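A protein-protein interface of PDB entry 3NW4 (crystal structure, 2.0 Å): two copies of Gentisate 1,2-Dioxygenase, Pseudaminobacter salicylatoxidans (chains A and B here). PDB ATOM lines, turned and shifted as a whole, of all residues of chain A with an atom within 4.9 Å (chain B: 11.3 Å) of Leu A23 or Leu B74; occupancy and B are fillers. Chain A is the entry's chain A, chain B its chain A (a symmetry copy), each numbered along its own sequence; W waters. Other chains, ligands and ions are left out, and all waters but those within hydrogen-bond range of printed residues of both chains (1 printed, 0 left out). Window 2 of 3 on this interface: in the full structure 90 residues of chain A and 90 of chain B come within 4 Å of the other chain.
OG1 of Thr A20 lies close to N of Glu A22 (3.4 Å). The backbone NH (N) of Leu A23 lies within hydrogen-bond range of the side-chain hydroxyl (OG1) of Thr A20 (3.1 Å). The backbone carbonyl oxygen (O) of Leu B67 is in hydrogen-bond range of the side-chain hydroxyl (OG) of Ser B71, at 2.7 Å. OE1 of Glu B73 lies within salt-bridge range of NZ of Lys B70 (3.2 Å). The backbone carbonyl oxygen (O) of Ser B71 sits at hydrogen-bond distance from the guanidinium group (NE) of Arg B84 (3.4 Å).
CB of Pro A17 touches O of Leu B74, 3.3 Å away. Glu A22 touches Leu B74. Leu A23 touches Leu B74. Leu A26 touches Lys B70. Leu A26 touches Ser B71.
Leu A23 touches one residue of chain B. No residue of chain B comes within 4 Å of Asp A19. No residue of chain B comes within 4 Å of Thr A20. No residue of chain B comes within 4 Å of Pro A21. Glu A22 touches just one residue of chain B: Leu B74. No residue of chain B comes within 4 Å of Arg A24. No residue of chain B comes within 4 Å of Tyr A27. Of the printed residues of chain A, Lys B70 touches Leu A26. Of the printed residues of chain B, Leu A26 touches Lys B70 and Ser B71. Printed residues of chain A within 4 Å of Ser B71: Leu A26 (3.7 Å). Glu B73 touches none of the printed residues of chain A. The nearest residue of chain B that does not touch Leu A23 is Val B75 (4.3 Å). The nearest residue of chain A that does not touch Leu B74 is Leu A26 (4.2 Å). The nearest printed residue of chain B that does not touch Leu A26 is Leu B67 (4.02 Å).
Hydrophobic or aromatic side chains of chain A that line the printed part of chain B: Pro A17 and Leu A26. Of the 21 printed residues of chain B, 3 touch a printed residue of chain A. Hydrophobic or aromatic side chains of chain B within 4 Å of the printed part of chain A: Leu B74. Along chain B the printed residues that touch a printed residue of chain A span positions 70 to 74. Among the printed residues, 5 pairs touch across the chains. Among the printed residues, no Asp or Glu carboxylate lies within 4 Å of a Lys or Arg side-chain nitrogen of the other chain.
No position is printed for both chains. Of the 5 pairs that touch across the chains among the printed residues, none has its exchanged pair printed and touching as well.
Water W1 bridges O of Leu B74 (2.8 Å) and N of Lys A18 (2.9 Å).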
ATOM      1  N   PRO A  17      -6.873 -15.231   3.217  1.00  0.00           N
ATOM      2  CA  PRO A  17      -5.492 -14.812   3.295  1.00  0.00           C
ATOM      3  C   PRO A  17      -4.561 -15.992   3.019  1.00  0.00           C
ATOM      4  O   PRO A  17      -4.957 -17.159   3.169  1.00  0.00           O
ATOM      5  CB  PRO A  17      -5.350 -14.353   4.742  1.00  0.00           C
ATOM      6  CG  PRO A  17      -6.333 -15.164   5.469  1.00  0.00           C
ATOM      7  CD  PRO A  17      -7.487 -15.358   4.546  1.00  0.00           C
ATOM      8  N   LYS A  18      -3.342 -15.671   2.620  1.00  0.00           N
ATOM      9  CA  LYS A  18      -2.303 -16.682   2.473  1.00  0.00           C
ATOM     10  C   LYS A  18      -1.967 -17.299   3.843  1.00  0.00           C
ATOM     11  O   LYS A  18      -1.763 -16.570   4.829  1.00  0.00           O
ATOM     12  CB  LYS A  18      -1.084 -16.023   1.868  1.00  0.00           C
ATOM     13  CG  LYS A  18      -1.253 -15.727   0.398  1.00  0.00           C
ATOM     14  CD  LYS A  18      -0.023 -14.974  -0.108  1.00  0.00           C
ATOM     15  CE  LYS A  18      -0.239 -14.501  -1.533  1.00  0.00           C
ATOM     16  NZ  LYS A  18       0.935 -13.651  -1.951  1.00  0.00           N
ATOM     17  N   ASP A  19      -1.937 -18.625   3.909  1.00  0.00           N
ATOM     18  CA  ASP A  19      -1.710 -19.320   5.168  1.00  0.00           C
ATOM     19  C   ASP A  19      -0.208 -19.391   5.498  1.00  0.00           C
ATOM     20  O   ASP A  19       0.477 -20.370   5.168  1.00  0.00           O
ATOM     21  CB  ASP A  19      -2.382 -20.691   5.133  1.00  0.00           C
ATOM     22  CG  ASP A  19      -2.272 -21.449   6.451  1.00  0.00           C
ATOM     23  OD1 ASP A  19      -2.517 -22.679   6.430  1.00  0.00           O
ATOM     24  OD2 ASP A  19      -1.946 -20.846   7.496  1.00  0.00           O
ATOM     25  N   THR A  20       0.279 -18.326   6.134  1.00  0.00           N
ATOM     26  CA  THR A  20       1.696 -18.137   6.451  1.00  0.00           C
ATOM     27  C   THR A  20       1.895 -18.091   7.969  1.00  0.00           C
ATOM     28  O   THR A  20       0.917 -17.956   8.704  1.00  0.00           O
ATOM     29  CB  THR A  20       2.188 -16.757   5.923  1.00  0.00           C
ATOM     30  OG1 THR A  20       1.394 -15.728   6.546  1.00  0.00           O
ATOM     31  CG2 THR A  20       2.042 -16.655   4.370  1.00  0.00           C
ATOM     32  N   PRO A  21       3.162 -18.168   8.445  1.00  0.00           N
ATOM     33  CA  PRO A  21       3.380 -18.025   9.882  1.00  0.00           C
ATOM     34  C   PRO A  21       2.851 -16.693  10.412  1.00  0.00           C
ATOM     35  O   PRO A  21       2.428 -16.629  11.556  1.00  0.00           O
ATOM     36  CB  PRO A  21       4.925 -18.065  10.020  1.00  0.00           C
ATOM     37  CG  PRO A  21       5.413 -18.832   8.831  1.00  0.00           C
ATOM     38  CD  PRO A  21       4.416 -18.506   7.723  1.00  0.00           C
ATOM     39  N   GLU A  22       2.913 -15.639   9.610  1.00  0.00           N
ATOM     40  CA  GLU A  22       2.457 -14.335  10.056  1.00  0.00           C
ATOM     41  C   GLU A  22       0.927 -14.339  10.211  1.00  0.00           C
ATOM     42  O   GLU A  22       0.407 -13.744  11.143  1.00  0.00           O
ATOM     43  CB  GLU A  22       2.909 -13.214   9.113  1.00  0.00           C
ATOM     44  CG  GLU A  22       4.454 -13.008   9.061  1.00  0.00           C
ATOM     45  CD  GLU A  22       5.240 -14.032   8.165  1.00  0.00           C
ATOM     46  OE1 GLU A  22       4.653 -14.900   7.475  1.00  0.00           O
ATOM     47  OE2 GLU A  22       6.493 -13.963   8.170  1.00  0.00           O
ATOM     48  N   LEU A  23       0.225 -15.021   9.311  1.00  0.00           N
ATOM     49  CA  LEU A  23      -1.224 -15.067   9.395  1.00  0.00           C
ATOM     50  C   LEU A  23      -1.595 -15.843  10.662  1.00  0.00           C
ATOM     51  O   LEU A  23      -2.406 -15.370  11.454  1.00  0.00           O
ATOM     52  CB  LEU A  23      -1.891 -15.688   8.149  1.00  0.00           C
ATOM     53  CG  LEU A  23      -3.415 -15.739   8.374  1.00  0.00           C
ATOM     54  CD1 LEU A  23      -4.079 -14.332   8.259  1.00  0.00           C
ATOM     55  CD2 LEU A  23      -4.124 -16.765   7.525  1.00  0.00           C
ATOM     56  N   ARG A  24      -0.984 -17.012  10.869  1.00  0.00           N
ATOM     57  CA  ARG A  24      -1.343 -17.869  12.010  1.00  0.00           C
ATOM     58  C   ARG A  24      -1.027 -17.137  13.328  1.00  0.00           C
ATOM     59  O   ARG A  24      -1.768 -17.298  14.291  1.00  0.00           O
ATOM     60  CB  ARG A  24      -0.631 -19.248  11.956  1.00  0.00           C
ATOM     61  CG  ARG A  24      -1.022 -20.077  10.736  1.00  0.00           C
ATOM     62  CD  ARG A  24      -0.419 -21.495  10.700  1.00  0.00           C
ATOM     63  NE  ARG A  24       1.036 -21.550  10.445  1.00  0.00           N
ATOM     64  CZ  ARG A  24       1.618 -21.530   9.232  1.00  0.00           C
ATOM     65  NH1 ARG A  24       0.891 -21.398   8.119  1.00  0.00           N
ATOM     66  NH2 ARG A  24       2.941 -21.611   9.130  1.00  0.00           N
ATOM     67  N   ALA A  25       0.051 -16.343  13.350  1.00  0.00           N
ATOM     68  CA  ALA A  25       0.404 -15.521  14.506  1.00  0.00           C
ATOM     69  C   ALA A  25      -0.673 -14.429  14.742  1.00  0.00           C
ATOM     70  O   ALA A  25      -1.062 -14.179  15.885  1.00  0.00           O
ATOM     71  CB  ALA A  25       1.802 -14.850  14.332  1.00  0.00           C
ATOM     72  N   LEU A  26      -1.088 -13.743  13.668  1.00  0.00           N
ATOM     73  CA  LEU A  26      -2.212 -12.821  13.763  1.00  0.00           C
ATOM     74  C   LEU A  26      -3.441 -13.526  14.392  1.00  0.00           C
ATOM     75  O   LEU A  26      -4.030 -13.015  15.351  1.00  0.00           O
ATOM     76  CB  LEU A  26      -2.564 -12.218  12.406  1.00  0.00           C
ATOM     77  CG  LEU A  26      -3.754 -11.245  12.408  1.00  0.00           C
ATOM     78  CD1 LEU A  26      -3.404 -10.020  13.276  1.00  0.00           C
ATOM     79  CD2 LEU A  26      -4.094 -10.820  10.983  1.00  0.00           C
ATOM     80  N   TYR A  27      -3.799 -14.705  13.889  1.00  0.00           N
ATOM     81  CA  TYR A  27      -4.986 -15.395  14.378  1.00  0.00           C
ATOM     82  C   TYR A  27      -4.823 -15.876  15.847  1.00  0.00           C
ATOM     83  O   TYR A  27      -5.826 -15.951  16.613  1.00  0.00           O
ATOM     84  CB  TYR A  27      -5.343 -16.556  13.472  1.00  0.00           C
ATOM     85  CG  TYR A  27      -6.037 -16.178  12.182  1.00  0.00           C
ATOM     86  CD1 TYR A  27      -6.170 -14.844  11.788  1.00  0.00           C
ATOM     87  CD2 TYR A  27      -6.525 -17.169  11.338  1.00  0.00           C
ATOM     88  CE1 TYR A  27      -6.788 -14.511  10.598  1.00  0.00           C
ATOM     89  CE2 TYR A  27      -7.150 -16.845  10.144  1.00  0.00           C
ATOM     90  CZ  TYR A  27      -7.269 -15.525   9.777  1.00  0.00           C
ATOM     91  OH  TYR A  27      -7.904 -15.206   8.602  1.00  0.00           O
ATOM     92  N   LEU B  65      -6.127  -1.326  17.280  1.00  0.00           N
ATOM     93  CA  LEU B  65      -5.459  -0.722  16.130  1.00  0.00           C
ATOM     94  C   LEU B  65      -4.331  -1.588  15.535  1.00  0.00           C
ATOM     95  O   LEU B  65      -4.235  -1.704  14.298  1.00  0.00           O
ATOM     96  CB  LEU B  65      -4.912   0.644  16.500  1.00  0.00           C
ATOM     97  CG  LEU B  65      -5.845   1.826  16.243  1.00  0.00           C
ATOM     98  CD1 LEU B  65      -5.127   3.096  16.605  1.00  0.00           C
ATOM     99  CD2 LEU B  65      -6.320   1.873  14.789  1.00  0.00           C
ATOM    100  N   ARG B  66      -3.511  -2.171  16.415  1.00  0.00           N
ATOM    101  CA  ARG B  66      -2.417  -3.076  16.031  1.00  0.00           C
ATOM    102  C   ARG B  66      -2.979  -4.278  15.258  1.00  0.00           C
ATOM    103  O   ARG B  66      -2.529  -4.569  14.157  1.00  0.00           O
ATOM    104  CB  ARG B  66      -1.659  -3.546  17.285  1.00  0.00           C
ATOM    105  CG  ARG B  66      -0.308  -4.294  17.004  1.00  0.00           C
ATOM    106  CD  ARG B  66       0.491  -4.517  18.305  1.00  0.00           C
ATOM    107  NE  ARG B  66      -0.188  -5.463  19.205  1.00  0.00           N
ATOM    108  CZ  ARG B  66      -0.713  -5.149  20.391  1.00  0.00           C
ATOM    109  NH1 ARG B  66      -0.641  -3.894  20.880  1.00  0.00           N
ATOM    110  NH2 ARG B  66      -1.305  -6.110  21.102  1.00  0.00           N
ATOM    111  N   LEU B  67      -3.968  -4.955  15.834  1.00  0.00           N
ATOM    112  CA  LEU B  67      -4.616  -6.116  15.194  1.00  0.00           C
ATOM    113  C   LEU B  67      -5.320  -5.742  13.870  1.00  0.00           C
ATOM    114  O   LEU B  67      -5.219  -6.461  12.866  1.00  0.00           O
ATOM    115  CB  LEU B  67      -5.590  -6.778  16.169  1.00  0.00           C
ATOM    116  CG  LEU B  67      -4.999  -7.296  17.494  1.00  0.00           C
ATOM    117  CD1 LEU B  67      -6.109  -7.663  18.465  1.00  0.00           C
ATOM    118  CD2 LEU B  67      -4.123  -8.503  17.285  1.00  0.00           C
ATOM    119  N   ALA B  68      -6.002  -4.600  13.855  1.00  0.00           N
ATOM    120  CA  ALA B  68      -6.669  -4.133  12.620  1.00  0.00           C
ATOM    121  C   ALA B  68      -5.647  -3.802  11.526  1.00  0.00           C
ATOM    122  O   ALA B  68      -5.847  -4.110  10.329  1.00  0.00           O
ATOM    123  CB  ALA B  68      -7.574  -2.918  12.914  1.00  0.00           C
ATOM    124  N   ARG B  69      -4.578  -3.140  11.935  1.00  0.00           N
ATOM    125  CA  ARG B  69      -3.531  -2.742  11.001  1.00  0.00           C
ATOM    126  C   ARG B  69      -2.835  -3.963  10.369  1.00  0.00           C
ATOM    127  O   ARG B  69      -2.616  -4.008   9.173  1.00  0.00           O
ATOM    128  CB  ARG B  69      -2.508  -1.823  11.669  1.00  0.00           C
ATOM    129  CG  ARG B  69      -2.881  -0.326  11.606  1.00  0.00           C
ATOM    130  CD  ARG B  69      -2.017   0.488  12.588  1.00  0.00           C
ATOM    131  NE  ARG B  69      -2.505   1.860  12.721  1.00  0.00           N
ATOM    132  CZ  ARG B  69      -2.217   2.681  13.727  1.00  0.00           C
ATOM    133  NH1 ARG B  69      -1.437   2.278  14.719  1.00  0.00           N
ATOM    134  NH2 ARG B  69      -2.718   3.915  13.740  1.00  0.00           N
ATOM    135  N   LYS B  70      -2.536  -4.957  11.189  1.00  0.00           N
ATOM    136  CA  LYS B  70      -1.916  -6.169  10.733  1.00  0.00           C
ATOM    137  C   LYS B  70      -2.879  -6.904   9.801  1.00  0.00           C
ATOM    138  O   LYS B  70      -2.462  -7.501   8.798  1.00  0.00           O
ATOM    139  CB  LYS B  70      -1.462  -6.998  11.957  1.00  0.00           C
ATOM    140  CG  LYS B  70      -0.775  -8.346  11.644  1.00  0.00           C
ATOM    141  CD  LYS B  70       0.466  -8.215  10.738  1.00  0.00           C
ATOM    142  CE  LYS B  70       1.560  -7.439  11.429  1.00  0.00           C
ATOM    143  NZ  LYS B  70       2.775  -7.493  10.580  1.00  0.00           N
ATOM    144  N   SER B  71      -4.172  -6.829  10.102  1.00  0.00           N
ATOM    145  CA  SER B  71      -5.205  -7.422   9.248  1.00  0.00           C
ATOM    146  C   SER B  71      -5.271  -6.744   7.896  1.00  0.00           C
ATOM    147  O   SER B  71      -5.477  -7.412   6.878  1.00  0.00           O
ATOM    148  CB  SER B  71      -6.590  -7.360   9.930  1.00  0.00           C
ATOM    149  OG  SER B  71      -6.537  -8.045  11.165  1.00  0.00           O
ATOM    150  N   GLY B  72      -5.093  -5.423   7.882  1.00  0.00           N
ATOM    151  CA  GLY B  72      -5.006  -4.674   6.639  1.00  0.00           C
ATOM    152  C   GLY B  72      -3.843  -5.155   5.759  1.00  0.00           C
ATOM    153  O   GLY B  72      -3.946  -5.110   4.531  1.00  0.00           O
ATOM    154  N   GLU B  73      -2.755  -5.619   6.382  1.00  0.00           N
ATOM    155  CA  GLU B  73      -1.585  -6.140   5.632  1.00  0.00           C
ATOM    156  C   GLU B  73      -1.838  -7.537   5.099  1.00  0.00           C
ATOM    157  O   GLU B  73      -1.493  -7.827   3.966  1.00  0.00           O
ATOM    158  CB  GLU B  73      -0.317  -6.207   6.503  1.00  0.00           C
ATOM    159  CG  GLU B  73       0.245  -4.847   6.918  1.00  0.00           C
ATOM    160  CD  GLU B  73       1.478  -4.972   7.811  1.00  0.00           C
ATOM    161  OE1 GLU B  73       2.168  -6.029   7.809  1.00  0.00           O
ATOM    162  OE2 GLU B  73       1.752  -3.991   8.527  1.00  0.00           O
ATOM    163  N   LEU B  74      -2.442  -8.396   5.915  1.00  0.00           N
ATOM    164  CA  LEU B  74      -2.503  -9.834   5.614  1.00  0.00           C
ATOM    165  C   LEU B  74      -3.810 -10.333   4.996  1.00  0.00           C
ATOM    166  O   LEU B  74      -3.849 -11.415   4.401  1.00  0.00           O
ATOM    167  CB  LEU B  74      -2.186 -10.623   6.880  1.00  0.00           C
ATOM    168  CG  LEU B  74      -0.841 -10.294   7.546  1.00  0.00           C
ATOM    169  CD1 LEU B  74      -0.615 -11.243   8.759  1.00  0.00           C
ATOM    170  CD2 LEU B  74       0.323 -10.410   6.523  1.00  0.00           C
ATOM    171  N   VAL B  75      -4.901  -9.605   5.118  1.00  0.00           N
ATOM    172  CA  VAL B  75      -6.168 -10.092   4.628  1.00  0.00           C
ATOM    173  C   VAL B  75      -6.794  -9.138   3.652  1.00  0.00           C
ATOM    174  O   VAL B  75      -7.061  -8.041   4.007  1.00  0.00           O
ATOM    175  CB  VAL B  75      -7.159 -10.271   5.766  1.00  0.00           C
ATOM    176  CG1 VAL B  75      -8.461 -10.688   5.265  1.00  0.00           C
ATOM    177  CG2 VAL B  75      -6.655 -11.142   6.826  1.00  0.00           C
ATOM    178  N   PRO B  76      -7.070  -9.568   2.429  1.00  0.00           N
ATOM    179  CA  PRO B  76      -7.746  -8.652   1.496  1.00  0.00           C
ATOM    180  C   PRO B  76      -9.239  -8.559   1.851  1.00  0.00           C
ATOM    181  O   PRO B  76      -9.810  -9.492   2.425  1.00  0.00           O
ATOM    182  CB  PRO B  76      -7.541  -9.310   0.141  1.00  0.00           C
ATOM    183  CG  PRO B  76      -7.499 -10.827   0.469  1.00  0.00           C
ATOM    184  CD  PRO B  76      -6.936 -10.943   1.900  1.00  0.00           C
ATOM    185  N   VAL B  77      -9.839  -7.420   1.540  1.00  0.00           N
ATOM    186  CA  VAL B  77     -11.268  -7.197   1.773  1.00  0.00           C
ATOM    187  C   VAL B  77     -11.978  -7.437   0.413  1.00  0.00           C
ATOM    188  O   VAL B  77     -11.433  -7.103  -0.644  1.00  0.00           O
ATOM    189  CB  VAL B  77     -11.524  -5.741   2.294  1.00  0.00           C
ATOM    190  CG1 VAL B  77     -11.047  -4.696   1.253  1.00  0.00           C
ATOM    191  CG2 VAL B  77     -13.002  -5.517   2.618  1.00  0.00           C
ATOM    192  N   GLY B  78     -13.171  -8.027   0.445  1.00  0.00           N
ATOM    193  CA  GLY B  78     -13.977  -8.172  -0.764  1.00  0.00           C
ATOM    194  C   GLY B  78     -15.111  -9.104  -0.481  1.00  0.00           C
ATOM    195  O   GLY B  78     -15.468  -9.311   0.696  1.00  0.00           O
ATOM    196  N   ARG B  83     -16.359  -7.768   4.850  1.00  0.00           N
ATOM    197  CA  ARG B  83     -15.783  -6.639   5.587  1.00  0.00           C
ATOM    198  C   ARG B  83     -14.570  -7.100   6.387  1.00  0.00           C
ATOM    199  O   ARG B  83     -14.580  -8.182   6.943  1.00  0.00           O
ATOM    200  CB  ARG B  83     -16.825  -6.076   6.599  1.00  0.00           C
ATOM    201  CG  ARG B  83     -18.217  -5.766   6.017  1.00  0.00           C
ATOM    202  CD  ARG B  83     -18.172  -4.555   5.125  1.00  0.00           C
ATOM    203  NE  ARG B  83     -19.464  -4.110   4.597  1.00  0.00           N
ATOM    204  CZ  ARG B  83     -19.855  -4.308   3.334  1.00  0.00           C
ATOM    205  NH1 ARG B  83     -19.056  -4.977   2.494  1.00  0.00           N
ATOM    206  NH2 ARG B  83     -21.018  -3.808   2.892  1.00  0.00           N
ATOM    207  N   ARG B  84     -13.529  -6.270   6.461  1.00  0.00           N
ATOM    208  CA  ARG B  84     -12.397  -6.546   7.346  1.00  0.00           C
ATOM    209  C   ARG B  84     -12.717  -5.984   8.746  1.00  0.00           C
ATOM    210  O   ARG B  84     -12.167  -4.955   9.165  1.00  0.00           O
ATOM    211  CB  ARG B  84     -11.107  -5.927   6.798  1.00  0.00           C
ATOM    212  CG  ARG B  84      -9.841  -6.388   7.503  1.00  0.00           C
ATOM    213  CD  ARG B  84      -8.603  -5.551   7.048  1.00  0.00           C
ATOM    214  NE  ARG B  84      -8.178  -5.805   5.647  1.00  0.00           N
ATOM    215  CZ  ARG B  84      -8.347  -4.989   4.592  1.00  0.00           C
ATOM    216  NH1 ARG B  84      -8.996  -3.835   4.698  1.00  0.00           N
ATOM    217  NH2 ARG B  84      -7.864  -5.340   3.394  1.00  0.00           N
ATOM    218  N   LEU B  86     -13.204  -6.754  12.895  1.00  0.00           N
ATOM    219  CA  LEU B  86     -12.690  -7.633  13.941  1.00  0.00           C
ATOM    220  C   LEU B  86     -13.666  -7.515  15.105  1.00  0.00           C
ATOM    221  O   LEU B  86     -13.698  -6.471  15.795  1.00  0.00           O
ATOM    222  CB  LEU B  86     -11.281  -7.185  14.386  1.00  0.00           C
ATOM    223  CG  LEU B  86     -10.008  -7.355  13.515  1.00  0.00           C
ATOM    224  CD1 LEU B  86     -10.152  -6.647  12.173  1.00  0.00           C
ATOM    225  CD2 LEU B  86      -8.771  -6.771  14.230  1.00  0.00           C
ATOM    226  N   TYR B 109     -11.450  -1.941   9.358  1.00  0.00           N
ATOM    227  CA  TYR B 109     -10.301  -1.251   8.781  1.00  0.00           C
ATOM    228  C   TYR B 109     -10.396  -1.289   7.256  1.00  0.00           C
ATOM    229  O   TYR B 109     -10.556  -2.354   6.655  1.00  0.00           O
ATOM    230  CB  TYR B 109      -9.026  -1.927   9.276  1.00  0.00           C
ATOM    231  CG  TYR B 109      -7.713  -1.325   8.806  1.00  0.00           C
ATOM    232  CD1 TYR B 109      -6.997  -0.426   9.598  1.00  0.00           C
ATOM    233  CD2 TYR B 109      -7.165  -1.699   7.583  1.00  0.00           C
ATOM    234  CE1 TYR B 109      -5.761   0.089   9.180  1.00  0.00           C
ATOM    235  CE2 TYR B 109      -5.949  -1.189   7.142  1.00  0.00           C
ATOM    236  CZ  TYR B 109      -5.247  -0.305   7.947  1.00  0.00           C
ATOM    237  OH  TYR B 109      -4.026   0.182   7.475  1.00  0.00           O
ATOM    238  N   GLY B 111      -8.291   0.017   3.909  1.00  0.00           N
ATOM    239  CA  GLY B 111      -7.032   0.593   3.461  1.00  0.00           C
ATOM    240  C   GLY B 111      -7.182   1.516   2.246  1.00  0.00           C
ATOM    241  O   GLY B 111      -8.265   1.652   1.668  1.00  0.00           O
ATOM    242  N   PRO B 112      -6.084   2.169   1.855  1.00  0.00           N
ATOM    243  CA  PRO B 112      -6.050   3.056   0.673  1.00  0.00           C
ATOM    244  C   PRO B 112      -6.845   2.504  -0.523  1.00  0.00           C
ATOM    245  O   PRO B 112      -6.606   1.371  -0.942  1.00  0.00           O
ATOM    246  CB  PRO B 112      -4.562   3.093   0.328  1.00  0.00           C
ATOM    247  CG  PRO B 112      -3.863   2.943   1.681  1.00  0.00           C
ATOM    248  CD  PRO B 112      -4.746   1.974   2.457  1.00  0.00           C
ATOM    249  N   GLU B 114      -9.467   1.008  -1.139  1.00  0.00           N
ATOM    250  CA  GLU B 114     -10.262  -0.216  -1.113  1.00  0.00           C
ATOM    251  C   GLU B 114     -11.754   0.089  -1.170  1.00  0.00           C
ATOM    252  O   GLU B 114     -12.180   1.149  -0.712  1.00  0.00           O
ATOM    253  CB  GLU B 114      -9.945  -1.040   0.120  1.00  0.00           C
ATOM    254  CG  GLU B 114      -8.507  -1.597   0.146  1.00  0.00           C
ATOM    255  CD  GLU B 114      -8.209  -2.346   1.443  1.00  0.00           C
ATOM    256  OE1 GLU B 114      -8.895  -2.116   2.470  1.00  0.00           O
ATOM    257  OE2 GLU B 114      -7.296  -3.190   1.429  1.00  0.00           O
HETATM  258  O   HOH W   1      -2.449 -12.892   2.551  1.00  0.00           O
